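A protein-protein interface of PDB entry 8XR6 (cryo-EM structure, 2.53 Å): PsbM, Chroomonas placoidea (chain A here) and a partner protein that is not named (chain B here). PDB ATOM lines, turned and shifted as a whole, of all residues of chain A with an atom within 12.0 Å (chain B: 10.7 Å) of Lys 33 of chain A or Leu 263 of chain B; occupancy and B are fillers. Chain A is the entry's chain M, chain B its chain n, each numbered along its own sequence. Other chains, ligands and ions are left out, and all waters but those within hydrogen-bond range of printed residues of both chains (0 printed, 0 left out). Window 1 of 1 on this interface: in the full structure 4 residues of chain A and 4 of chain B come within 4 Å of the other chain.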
ATOM      1  N   LEU A  22     -11.841  12.402   3.753  1.00  0.00           N
ATOM      2  CA  LEU A  22     -12.472  13.231   4.777  1.00  0.00           C
ATOM      3  C   LEU A  22     -13.192  14.423   4.161  1.00  0.00           C
ATOM      4  O   LEU A  22     -14.307  14.764   4.575  1.00  0.00           O
ATOM      5  CB  LEU A  22     -11.419  13.707   5.774  1.00  0.00           C
ATOM      6  CG  LEU A  22     -10.855  12.640   6.707  1.00  0.00           C
ATOM      7  CD1 LEU A  22      -9.513  13.087   7.236  1.00  0.00           C
ATOM      8  CD2 LEU A  22     -11.816  12.368   7.850  1.00  0.00           C
ATOM      9  N   VAL A  23     -12.568  15.075   3.180  1.00  0.00           N
ATOM     10  CA  VAL A  23     -13.189  16.232   2.546  1.00  0.00           C
ATOM     11  C   VAL A  23     -14.471  15.821   1.831  1.00  0.00           C
ATOM     12  O   VAL A  23     -15.477  16.537   1.875  1.00  0.00           O
ATOM     13  CB  VAL A  23     -12.192  16.915   1.591  1.00  0.00           C
ATOM     14  CG1 VAL A  23     -12.892  17.951   0.727  1.00  0.00           C
ATOM     15  CG2 VAL A  23     -11.069  17.569   2.380  1.00  0.00           C
ATOM     16  N   THR A  24     -14.456  14.668   1.161  1.00  0.00           N
ATOM     17  CA  THR A  24     -15.660  14.174   0.506  1.00  0.00           C
ATOM     18  C   THR A  24     -16.749  13.859   1.523  1.00  0.00           C
ATOM     19  O   THR A  24     -17.923  14.176   1.300  1.00  0.00           O
ATOM     20  CB  THR A  24     -15.328  12.933  -0.323  1.00  0.00           C
ATOM     21  OG1 THR A  24     -14.316  13.255  -1.285  1.00  0.00           O
ATOM     22  CG2 THR A  24     -16.561  12.422  -1.048  1.00  0.00           C
ATOM     23  N   LEU A  25     -16.383  13.229   2.642  1.00  0.00           N
ATOM     24  CA  LEU A  25     -17.379  12.913   3.662  1.00  0.00           C
ATOM     25  C   LEU A  25     -17.980  14.181   4.256  1.00  0.00           C
ATOM     26  O   LEU A  25     -19.158  14.209   4.626  1.00  0.00           O
ATOM     27  CB  LEU A  25     -16.763  12.053   4.768  1.00  0.00           C
ATOM     28  CG  LEU A  25     -16.979  10.536   4.766  1.00  0.00           C
ATOM     29  CD1 LEU A  25     -16.342   9.948   6.010  1.00  0.00           C
ATOM     30  CD2 LEU A  25     -18.451  10.150   4.703  1.00  0.00           C
ATOM     31  N   TYR A  26     -17.189  15.250   4.347  1.00  0.00           N
ATOM     32  CA  TYR A  26     -17.729  16.509   4.855  1.00  0.00           C
ATOM     33  C   TYR A  26     -18.637  17.181   3.827  1.00  0.00           C
ATOM     34  O   TYR A  26     -19.701  17.712   4.175  1.00  0.00           O
ATOM     35  CB  TYR A  26     -16.594  17.449   5.250  1.00  0.00           C
ATOM     36  CG  TYR A  26     -17.080  18.818   5.655  1.00  0.00           C
ATOM     37  CD1 TYR A  26     -17.845  18.992   6.799  1.00  0.00           C
ATOM     38  CD2 TYR A  26     -16.784  19.935   4.891  1.00  0.00           C
ATOM     39  CE1 TYR A  26     -18.295  20.237   7.171  1.00  0.00           C
ATOM     40  CE2 TYR A  26     -17.229  21.186   5.258  1.00  0.00           C
ATOM     41  CZ  TYR A  26     -17.985  21.331   6.398  1.00  0.00           C
ATOM     42  OH  TYR A  26     -18.433  22.576   6.765  1.00  0.00           O
ATOM     43  N   ILE A  27     -18.223  17.188   2.560  1.00  0.00           N
ATOM     44  CA  ILE A  27     -18.973  17.914   1.538  1.00  0.00           C
ATOM     45  C   ILE A  27     -20.286  17.206   1.228  1.00  0.00           C
ATOM     46  O   ILE A  27     -21.319  17.856   1.036  1.00  0.00           O
ATOM     47  CB  ILE A  27     -18.110  18.103   0.277  1.00  0.00           C
ATOM     48  CG1 ILE A  27     -16.968  19.086   0.562  1.00  0.00           C
ATOM     49  CG2 ILE A  27     -18.964  18.603  -0.889  1.00  0.00           C
ATOM     50  CD1 ILE A  27     -15.839  19.049  -0.447  1.00  0.00           C
ATOM     51  N   GLN A  28     -20.253  15.892   1.196  1.00  0.00           N
ATOM     52  CA  GLN A  28     -21.446  15.117   0.970  1.00  0.00           C
ATOM     53  C   GLN A  28     -22.476  15.472   2.024  1.00  0.00           C
ATOM     54  O   GLN A  28     -23.625  15.753   1.717  1.00  0.00           O
ATOM     55  CB  GLN A  28     -21.028  13.651   1.038  1.00  0.00           C
ATOM     56  CG  GLN A  28     -22.071  12.626   1.406  1.00  0.00           C
ATOM     57  CD  GLN A  28     -22.250  12.464   2.893  1.00  0.00           C
ATOM     58  OE1 GLN A  28     -21.285  12.297   3.636  1.00  0.00           O
ATOM     59  NE2 GLN A  28     -23.496  12.523   3.339  1.00  0.00           N
ATOM     60  N   SER A  29     -22.050  15.446   3.280  1.00  0.00           N
ATOM     61  CA  SER A  29     -22.924  15.656   4.424  1.00  0.00           C
ATOM     62  C   SER A  29     -23.522  17.034   4.427  1.00  0.00           C
ATOM     63  O   SER A  29     -24.692  17.203   4.741  1.00  0.00           O
ATOM     64  CB  SER A  29     -22.145  15.439   5.713  1.00  0.00           C
ATOM     65  OG  SER A  29     -21.111  16.392   5.847  1.00  0.00           O
ATOM     66  N   GLU A  30     -22.722  18.025   4.079  1.00  0.00           N
ATOM     67  CA  GLU A  30     -23.202  19.386   4.041  1.00  0.00           C
ATOM     68  C   GLU A  30     -24.195  19.533   2.922  1.00  0.00           C
ATOM     69  O   GLU A  30     -25.282  20.057   3.123  1.00  0.00           O
ATOM     70  CB  GLU A  30     -22.039  20.337   3.838  1.00  0.00           C
ATOM     71  CG  GLU A  30     -20.992  20.289   4.927  1.00  0.00           C
ATOM     72  CD  GLU A  30     -21.599  20.263   6.309  1.00  0.00           C
ATOM     73  OE1 GLU A  30     -21.650  19.175   6.920  1.00  0.00           O
ATOM     74  OE2 GLU A  30     -22.024  21.335   6.782  1.00  0.00           O
ATOM     75  N   SER A  31     -23.840  19.057   1.745  1.00  0.00           N
ATOM     76  CA  SER A  31     -24.759  19.097   0.637  1.00  0.00           C
ATOM     77  C   SER A  31     -26.098  18.521   1.055  1.00  0.00           C
ATOM     78  O   SER A  31     -27.134  19.113   0.800  1.00  0.00           O
ATOM     79  CB  SER A  31     -24.182  18.328  -0.538  1.00  0.00           C
ATOM     80  OG  SER A  31     -25.083  18.310  -1.627  1.00  0.00           O
ATOM     81  N   ARG A  32     -26.081  17.370   1.714  1.00  0.00           N
ATOM     82  CA  ARG A  32     -27.331  16.748   2.138  1.00  0.00           C
ATOM     83  C   ARG A  32     -28.093  17.645   3.106  1.00  0.00           C
ATOM     84  O   ARG A  32     -29.324  17.759   3.022  1.00  0.00           O
ATOM     85  CB  ARG A  32     -27.056  15.386   2.772  1.00  0.00           C
ATOM     86  CG  ARG A  32     -28.212  14.404   2.638  1.00  0.00           C
ATOM     87  CD  ARG A  32     -27.827  13.019   3.121  1.00  0.00           C
ATOM     88  NE  ARG A  32     -28.723  11.978   2.629  1.00  0.00           N
ATOM     89  CZ  ARG A  32     -29.966  11.785   3.050  1.00  0.00           C
ATOM     90  NH1 ARG A  32     -30.522  12.563   3.965  1.00  0.00           N
ATOM     91  NH2 ARG A  32     -30.672  10.780   2.540  1.00  0.00           N
ATOM     92  N   LYS A  33     -27.380  18.293   4.033  1.00  0.00           N
ATOM     93  CA  LYS A  33     -28.034  19.212   4.961  1.00  0.00           C
ATOM     94  C   LYS A  33     -28.683  20.369   4.216  1.00  0.00           C
ATOM     95  O   LYS A  33     -29.817  20.758   4.516  1.00  0.00           O
ATOM     96  CB  LYS A  33     -27.030  19.737   5.987  1.00  0.00           C
ATOM     97  CG  LYS A  33     -27.022  18.969   7.300  1.00  0.00           C
ATOM     98  CD  LYS A  33     -25.676  19.004   8.030  1.00  0.00           C
ATOM     99  CE  LYS A  33     -25.223  20.410   8.427  1.00  0.00           C
ATOM    100  NZ  LYS A  33     -23.748  20.471   8.617  1.00  0.00           N
ATOM    101  N   ALA A  34     -27.975  20.934   3.236  1.00  0.00           N
ATOM    102  CA  ALA A  34     -28.552  22.011   2.439  1.00  0.00           C
ATOM    103  C   ALA A  34     -29.743  21.529   1.621  1.00  0.00           C
ATOM    104  O   ALA A  34     -30.739  22.252   1.494  1.00  0.00           O
ATOM    105  CB  ALA A  34     -27.489  22.610   1.522  1.00  0.00           C
ATOM    106  N   GLY A  35     -29.662  20.322   1.064  1.00  0.00           N
ATOM    107  CA  GLY A  35     -30.760  19.804   0.266  1.00  0.00           C
ATOM    108  C   GLY A  35     -32.005  19.536   1.086  1.00  0.00           C
ATOM    109  O   GLY A  35     -33.126  19.655   0.582  1.00  0.00           O
ATOM    110  N   SER A  36     -31.830  19.150   2.354  1.00  0.00           N
ATOM    111  CA  SER A  36     -32.988  18.901   3.208  1.00  0.00           C
ATOM    112  C   SER A  36     -33.831  20.159   3.377  1.00  0.00           C
ATOM    113  O   SER A  36     -35.065  20.098   3.347  1.00  0.00           O
ATOM    114  CB  SER A  36     -32.533  18.379   4.570  1.00  0.00           C
ATOM    115  OG  SER A  36     -31.886  19.397   5.312  1.00  0.00           O
ATOM    116  N   SER A  37     -33.185  21.306   3.553  1.00  0.00           N
ATOM    117  CA  SER A  37     -33.898  22.574   3.669  1.00  0.00           C
ATOM    118  C   SER A  37     -34.346  23.073   2.300  1.00  0.00           C
ATOM    119  O   SER A  37     -33.813  24.055   1.781  1.00  0.00           O
ATOM    120  CB  SER A  37     -33.020  23.624   4.350  1.00  0.00           C
ATOM    121  OG  SER A  37     -32.221  24.312   3.403  1.00  0.00           O
ATOM    122  N   GLY B 255     -27.732  31.806  14.186  1.00  0.00           N
ATOM    123  CA  GLY B 255     -26.481  31.854  13.448  1.00  0.00           C
ATOM    124  C   GLY B 255     -25.943  30.504  13.030  1.00  0.00           C
ATOM    125  O   GLY B 255     -25.093  30.441  12.129  1.00  0.00           O
ATOM    126  N   ASN B 256     -26.399  29.415  13.653  1.00  0.00           N
ATOM    127  CA  ASN B 256     -25.958  28.065  13.294  1.00  0.00           C
ATOM    128  C   ASN B 256     -27.038  27.078  13.722  1.00  0.00           C
ATOM    129  O   ASN B 256     -26.868  26.318  14.682  1.00  0.00           O
ATOM    130  CB  ASN B 256     -24.614  27.741  13.946  1.00  0.00           C
ATOM    131  CG  ASN B 256     -23.931  26.539  13.321  1.00  0.00           C
ATOM    132  OD1 ASN B 256     -24.338  26.051  12.267  1.00  0.00           O
ATOM    133  ND2 ASN B 256     -22.882  26.056  13.971  1.00  0.00           N
ATOM    134  N   PRO B 257     -28.180  27.066  13.022  1.00  0.00           N
ATOM    135  CA  PRO B 257     -29.318  26.253  13.482  1.00  0.00           C
ATOM    136  C   PRO B 257     -29.067  24.754  13.482  1.00  0.00           C
ATOM    137  O   PRO B 257     -29.791  24.030  14.175  1.00  0.00           O
ATOM    138  CB  PRO B 257     -30.428  26.627  12.488  1.00  0.00           C
ATOM    139  CG  PRO B 257     -29.707  27.033  11.263  1.00  0.00           C
ATOM    140  CD  PRO B 257     -28.476  27.737  11.744  1.00  0.00           C
ATOM    141  N   SER B 258     -28.073  24.262  12.740  1.00  0.00           N
ATOM    142  CA  SER B 258     -27.799  22.836  12.646  1.00  0.00           C
ATOM    143  C   SER B 258     -26.764  22.346  13.648  1.00  0.00           C
ATOM    144  O   SER B 258     -26.404  21.162  13.608  1.00  0.00           O
ATOM    145  CB  SER B 258     -27.329  22.486  11.226  1.00  0.00           C
ATOM    146  OG  SER B 258     -26.325  23.384  10.788  1.00  0.00           O
ATOM    147  N   PHE B 259     -26.276  23.202  14.544  1.00  0.00           N
ATOM    148  CA  PHE B 259     -25.229  22.787  15.466  1.00  0.00           C
ATOM    149  C   PHE B 259     -25.758  21.769  16.467  1.00  0.00           C
ATOM    150  O   PHE B 259     -26.876  21.899  16.974  1.00  0.00           O
ATOM    151  CB  PHE B 259     -24.662  23.990  16.212  1.00  0.00           C
ATOM    152  CG  PHE B 259     -23.398  23.683  16.956  1.00  0.00           C
ATOM    153  CD1 PHE B 259     -22.185  23.636  16.292  1.00  0.00           C
ATOM    154  CD2 PHE B 259     -23.425  23.412  18.315  1.00  0.00           C
ATOM    155  CE1 PHE B 259     -21.024  23.342  16.970  1.00  0.00           C
ATOM    156  CE2 PHE B 259     -22.264  23.114  18.995  1.00  0.00           C
ATOM    157  CZ  PHE B 259     -21.062  23.080  18.319  1.00  0.00           C
ATOM    158  N   GLY B 260     -24.941  20.762  16.759  1.00  0.00           N
ATOM    159  CA  GLY B 260     -25.290  19.751  17.731  1.00  0.00           C
ATOM    160  C   GLY B 260     -26.360  18.781  17.288  1.00  0.00           C
ATOM    161  O   GLY B 260     -26.889  18.045  18.132  1.00  0.00           O
ATOM    162  N   LYS B 261     -26.699  18.757  15.999  1.00  0.00           N
ATOM    163  CA  LYS B 261     -27.746  17.902  15.461  1.00  0.00           C
ATOM    164  C   LYS B 261     -27.179  17.042  14.344  1.00  0.00           C
ATOM    165  O   LYS B 261     -26.384  17.511  13.524  1.00  0.00           O
ATOM    166  CB  LYS B 261     -28.921  18.728  14.932  1.00  0.00           C
ATOM    167  CG  LYS B 261     -29.371  19.837  15.866  1.00  0.00           C
ATOM    168  CD  LYS B 261     -30.644  20.496  15.367  1.00  0.00           C
ATOM    169  CE  LYS B 261     -31.265  21.407  16.416  1.00  0.00           C
ATOM    170  NZ  LYS B 261     -31.263  22.830  15.982  1.00  0.00           N
ATOM    171  N   SER B 262     -27.593  15.781  14.321  1.00  0.00           N
ATOM    172  CA  SER B 262     -27.161  14.859  13.286  1.00  0.00           C
ATOM    173  C   SER B 262     -27.859  15.175  11.967  1.00  0.00           C
ATOM    174  O   SER B 262     -28.741  16.035  11.892  1.00  0.00           O
ATOM    175  CB  SER B 262     -27.452  13.421  13.716  1.00  0.00           C
ATOM    176  OG  SER B 262     -28.668  12.958  13.159  1.00  0.00           O
ATOM    177  N   LEU B 263     -27.437  14.478  10.907  1.00  0.00           N
ATOM    178  CA  LEU B 263     -28.110  14.612   9.617  1.00  0.00           C
ATOM    179  C   LEU B 263     -29.587  14.269   9.734  1.00  0.00           C
ATOM    180  O   LEU B 263     -30.450  15.017   9.265  1.00  0.00           O
ATOM    181  CB  LEU B 263     -27.460  13.708   8.561  1.00  0.00           C
ATOM    182  CG  LEU B 263     -26.533  14.291   7.487  1.00  0.00           C
ATOM    183  CD1 LEU B 263     -25.945  13.165   6.633  1.00  0.00           C
ATOM    184  CD2 LEU B 263     -27.254  15.295   6.585  1.00  0.00           C
ATOM    185  N   ILE B 264     -29.897  13.135  10.360  1.00  0.00           N
ATOM    186  CA  ILE B 264     -31.280  12.673  10.423  1.00  0.00           C
ATOM    187  C   ILE B 264     -32.110  13.601  11.301  1.00  0.00           C
ATOM    188  O   ILE B 264     -33.240  13.965  10.951  1.00  0.00           O
ATOM    189  CB  ILE B 264     -31.331  11.216  10.919  1.00  0.00           C
ATOM    190  CG1 ILE B 264     -30.726  10.286   9.859  1.00  0.00           C
ATOM    191  CG2 ILE B 264     -32.775  10.811  11.248  1.00  0.00           C
ATOM    192  CD1 ILE B 264     -30.448   8.877  10.341  1.00  0.00           C
ATOM    193  N   GLU B 265     -31.563  14.001  12.450  1.00  0.00           N
ATOM    194  CA  GLU B 265     -32.299  14.865  13.368  1.00  0.00           C
ATOM    195  C   GLU B 265     -32.607  16.210  12.723  1.00  0.00           C
ATOM    196  O   GLU B 265     -33.756  16.667  12.716  1.00  0.00           O
ATOM    197  CB  GLU B 265     -31.491  15.044  14.658  1.00  0.00           C
ATOM    198  CG  GLU B 265     -31.967  16.167  15.576  1.00  0.00           C
ATOM    199  CD  GLU B 265     -31.290  16.130  16.932  1.00  0.00           C
ATOM    200  OE1 GLU B 265     -30.299  15.386  17.085  1.00  0.00           O
ATOM    201  OE2 GLU B 265     -31.748  16.848  17.846  1.00  0.00           O
ATOM    202  N   TYR B 266     -31.584  16.857  12.159  1.00  0.00           N
ATOM    203  CA  TYR B 266     -31.791  18.160  11.538  1.00  0.00           C
ATOM    204  C   TYR B 266     -32.671  18.055  10.300  1.00  0.00           C
ATOM    205  O   TYR B 266     -33.464  18.961  10.025  1.00  0.00           O
ATOM    206  CB  TYR B 266     -30.444  18.789  11.187  1.00  0.00           C
ATOM    207  CG  TYR B 266     -30.550  20.178  10.604  1.00  0.00           C
ATOM    208  CD1 TYR B 266     -31.042  21.233  11.358  1.00  0.00           C
ATOM    209  CD2 TYR B 266     -30.146  20.437   9.302  1.00  0.00           C
ATOM    210  CE1 TYR B 266     -31.138  22.504  10.831  1.00  0.00           C
ATOM    211  CE2 TYR B 266     -30.236  21.705   8.768  1.00  0.00           C
ATOM    212  CZ  TYR B 266     -30.733  22.736   9.536  1.00  0.00           C
ATOM    213  OH  TYR B 266     -30.825  24.003   9.009  1.00  0.00           O
ATOM    214  N   SER B 267     -32.545  16.963   9.541  1.00  0.00           N
ATOM    215  CA  SER B 267     -33.397  16.773   8.374  1.00  0.00           C
ATOM    216  C   SER B 267     -34.860  16.641   8.776  1.00  0.00           C
ATOM    217  O   SER B 267     -35.737  17.269   8.172  1.00  0.00           O
ATOM    218  CB  SER B 267     -32.947  15.538   7.594  1.00  0.00           C
ATOM    219  OG  SER B 267     -33.957  15.106   6.700  1.00  0.00           O
ATOM    220  N   GLU B 268     -35.143  15.834   9.800  1.00  0.00           N
ATOM    221  CA  GLU B 268     -36.520  15.689  10.257  1.00  0.00           C
ATOM    222  C   GLU B 268     -37.044  16.983  10.861  1.00  0.00           C
ATOM    223  O   GLU B 268     -38.242  17.273  10.754  1.00  0.00           O
ATOM    224  CB  GLU B 268     -36.622  14.546  11.267  1.00  0.00           C
ATOM    225  CG  GLU B 268     -36.388  13.172  10.658  1.00  0.00           C
ATOM    226  CD  GLU B 268     -36.423  12.060  11.688  1.00  0.00           C
ATOM    227  OE1 GLU B 268     -36.962  12.287  12.791  1.00  0.00           O
ATOM    228  OE2 GLU B 268     -35.910  10.961  11.393  1.00  0.00           O
ATOM    229  N   GLU B 269     -36.172  17.787  11.438  1.00  0.00           N
ATOM    230  CA  GLU B 269     -36.593  19.072  11.976  1.00  0.00           C
ATOM    231  C   GLU B 269     -36.961  20.017  10.863  1.00  0.00           C
ATOM    232  O   GLU B 269     -37.986  20.673  10.924  1.00  0.00           O
ATOM    233  CB  GLU B 269     -35.469  19.680  12.813  1.00  0.00           C
ATOM    234  CG  GLU B 269     -35.300  21.182  12.660  1.00  0.00           C
ATOM    235  CD  GLU B 269     -34.156  21.725  13.491  1.00  0.00           C
ATOM    236  OE1 GLU B 269     -33.505  20.932  14.198  1.00  0.00           O
ATOM    237  OE2 GLU B 269     -33.901  22.945  13.433  1.00  0.00           O
ATOM    238  N   THR B 270     -36.114  20.111   9.851  1.00  0.00           N
ATOM    239  CA  THR B 270     -36.353  21.039   8.749  1.00  0.00           C
ATOM    240  C   THR B 270     -37.631  20.717   7.985  1.00  0.00           C
ATOM    241  O   THR B 270     -38.234  21.627   7.405  1.00  0.00           O
ATOM    242  CB  THR B 270     -35.167  21.037   7.784  1.00  0.00           C
ATOM    243  OG1 THR B 270     -34.812  19.688   7.459  1.00  0.00           O
ATOM    244  CG2 THR B 270     -33.971  21.746   8.403  1.00  0.00           C
ATOM    245  N   LYS B 271     -38.051  19.453   7.968  1.00  0.00           N
ATOM    246  CA  LYS B 271     -39.330  19.056   7.394  1.00  0.00           C
ATOM    247  C   LYS B 271     -40.481  19.191   8.390  1.00  0.00           C
ATOM    248  O   LYS B 271     -41.630  18.902   8.036  1.00  0.00           O
ATOM    249  CB  LYS B 271     -39.244  17.621   6.869  1.00  0.00           C
ATOM    250  CG  LYS B 271     -38.296  17.453   5.687  1.00  0.00           C
ATOM    251  CD  LYS B 271     -37.632  16.083   5.678  1.00  0.00           C
ATOM    252  CE  LYS B 271     -36.893  15.835   4.371  1.00  0.00           C
ATOM    253  NZ  LYS B 271     -36.019  14.631   4.435  1.00  0.00           N
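Of the 16 printed residues of chain A, 4 touch a printed residue of chain B.
Printed residues of chain A that touch a printed residue of chain B: Ser 29, Arg 32, Lys 33 and Ser 36.
Of the 17 printed residues of chain B, 4 touch a printed residue of chain A.
Among the printed residues, 6 pairs touch across the chains.
Among the printed residues, merely in contact across the chains: Ser 36 of chain A with Thr 270 of chain B (3.6 Å), Ser 29 of chain A with Leu 263 of chain B (3.7 Å), Lys 33 of chain A with Leu 263 of chain B (3.8 Å), Arg 32 of chain A with Leu 263 of chain B (3.8 Å), Lys 33 of chain A with Ser 258 of chain B (3.95 Å) and Lys 33 of chain A with Tyr 266 of chain B (3.99 Å).
Of the printed residues of chain B, Lys 33 of chain A touches Ser 258, Leu 263 and Tyr 266.
Of chain A, only Ser 29 (3.7 Å), Arg 32 (3.8 Å) and Lys 33 (3.8 Å) come within 4 Å of Leu 263 of chain B.
No residue of chain B comes within 4 Å of Glu 30 of chain A.
No residue of chain B comes within 4 Å of Ala 34 of chain A.
Ser 36 of chain A touches one residue of chain B.
Ser 37 of chain A touches none of the printed residues of chain B.
No residue of chain A comes within 4 Å of Ser 262 of chain B.
No residue of chain A comes within 4 Å of Ser 267 of chain B.
Printed residues of chain A within 4 Å of Tyr 266 of chain B: Lys 33 (3.99 Å).
Of the printed residues of chain A, Thr 270 of chain B touches Ser 36 (3.6 Å).
Printed residues of chain B within 4 Å of Arg 32 of chain A: Leu 263 (3.8 Å).
Thr 24 of chain A touches none of the printed residues of chain B.
O of Tyr 266 of chain B sits at hydrogen-bond distance from OG1 of Thr 270 of chain B (3.0 Å).
The backbone carbonyl oxygen of Tyr 26 of chain A lies within hydrogen-bond range of the side-chain hydroxyl of Ser 29 of chain A, at 2.6 Å.
The backbone carbonyl oxygen (O) of Ser 267 of chain B lies within hydrogen-bond range of the side-chain hydroxyl (OG1) of Thr 270 of chain B (2.7 Å).
O of Lys 33 of chain A sits at hydrogen-bond distance from OG of Ser 36 of chain A, at 2.6 Å.
OE1 of Glu 30 of chain A sits at hydrogen-bond distance from OG of Ser 29 of chain A (3.0 Å).
The side-chain carboxylate (OE2) of Glu 30 of chain A lies within salt-bridge range of the side-chain amino group (NZ) of Lys 33 of chain A (2.7 Å).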
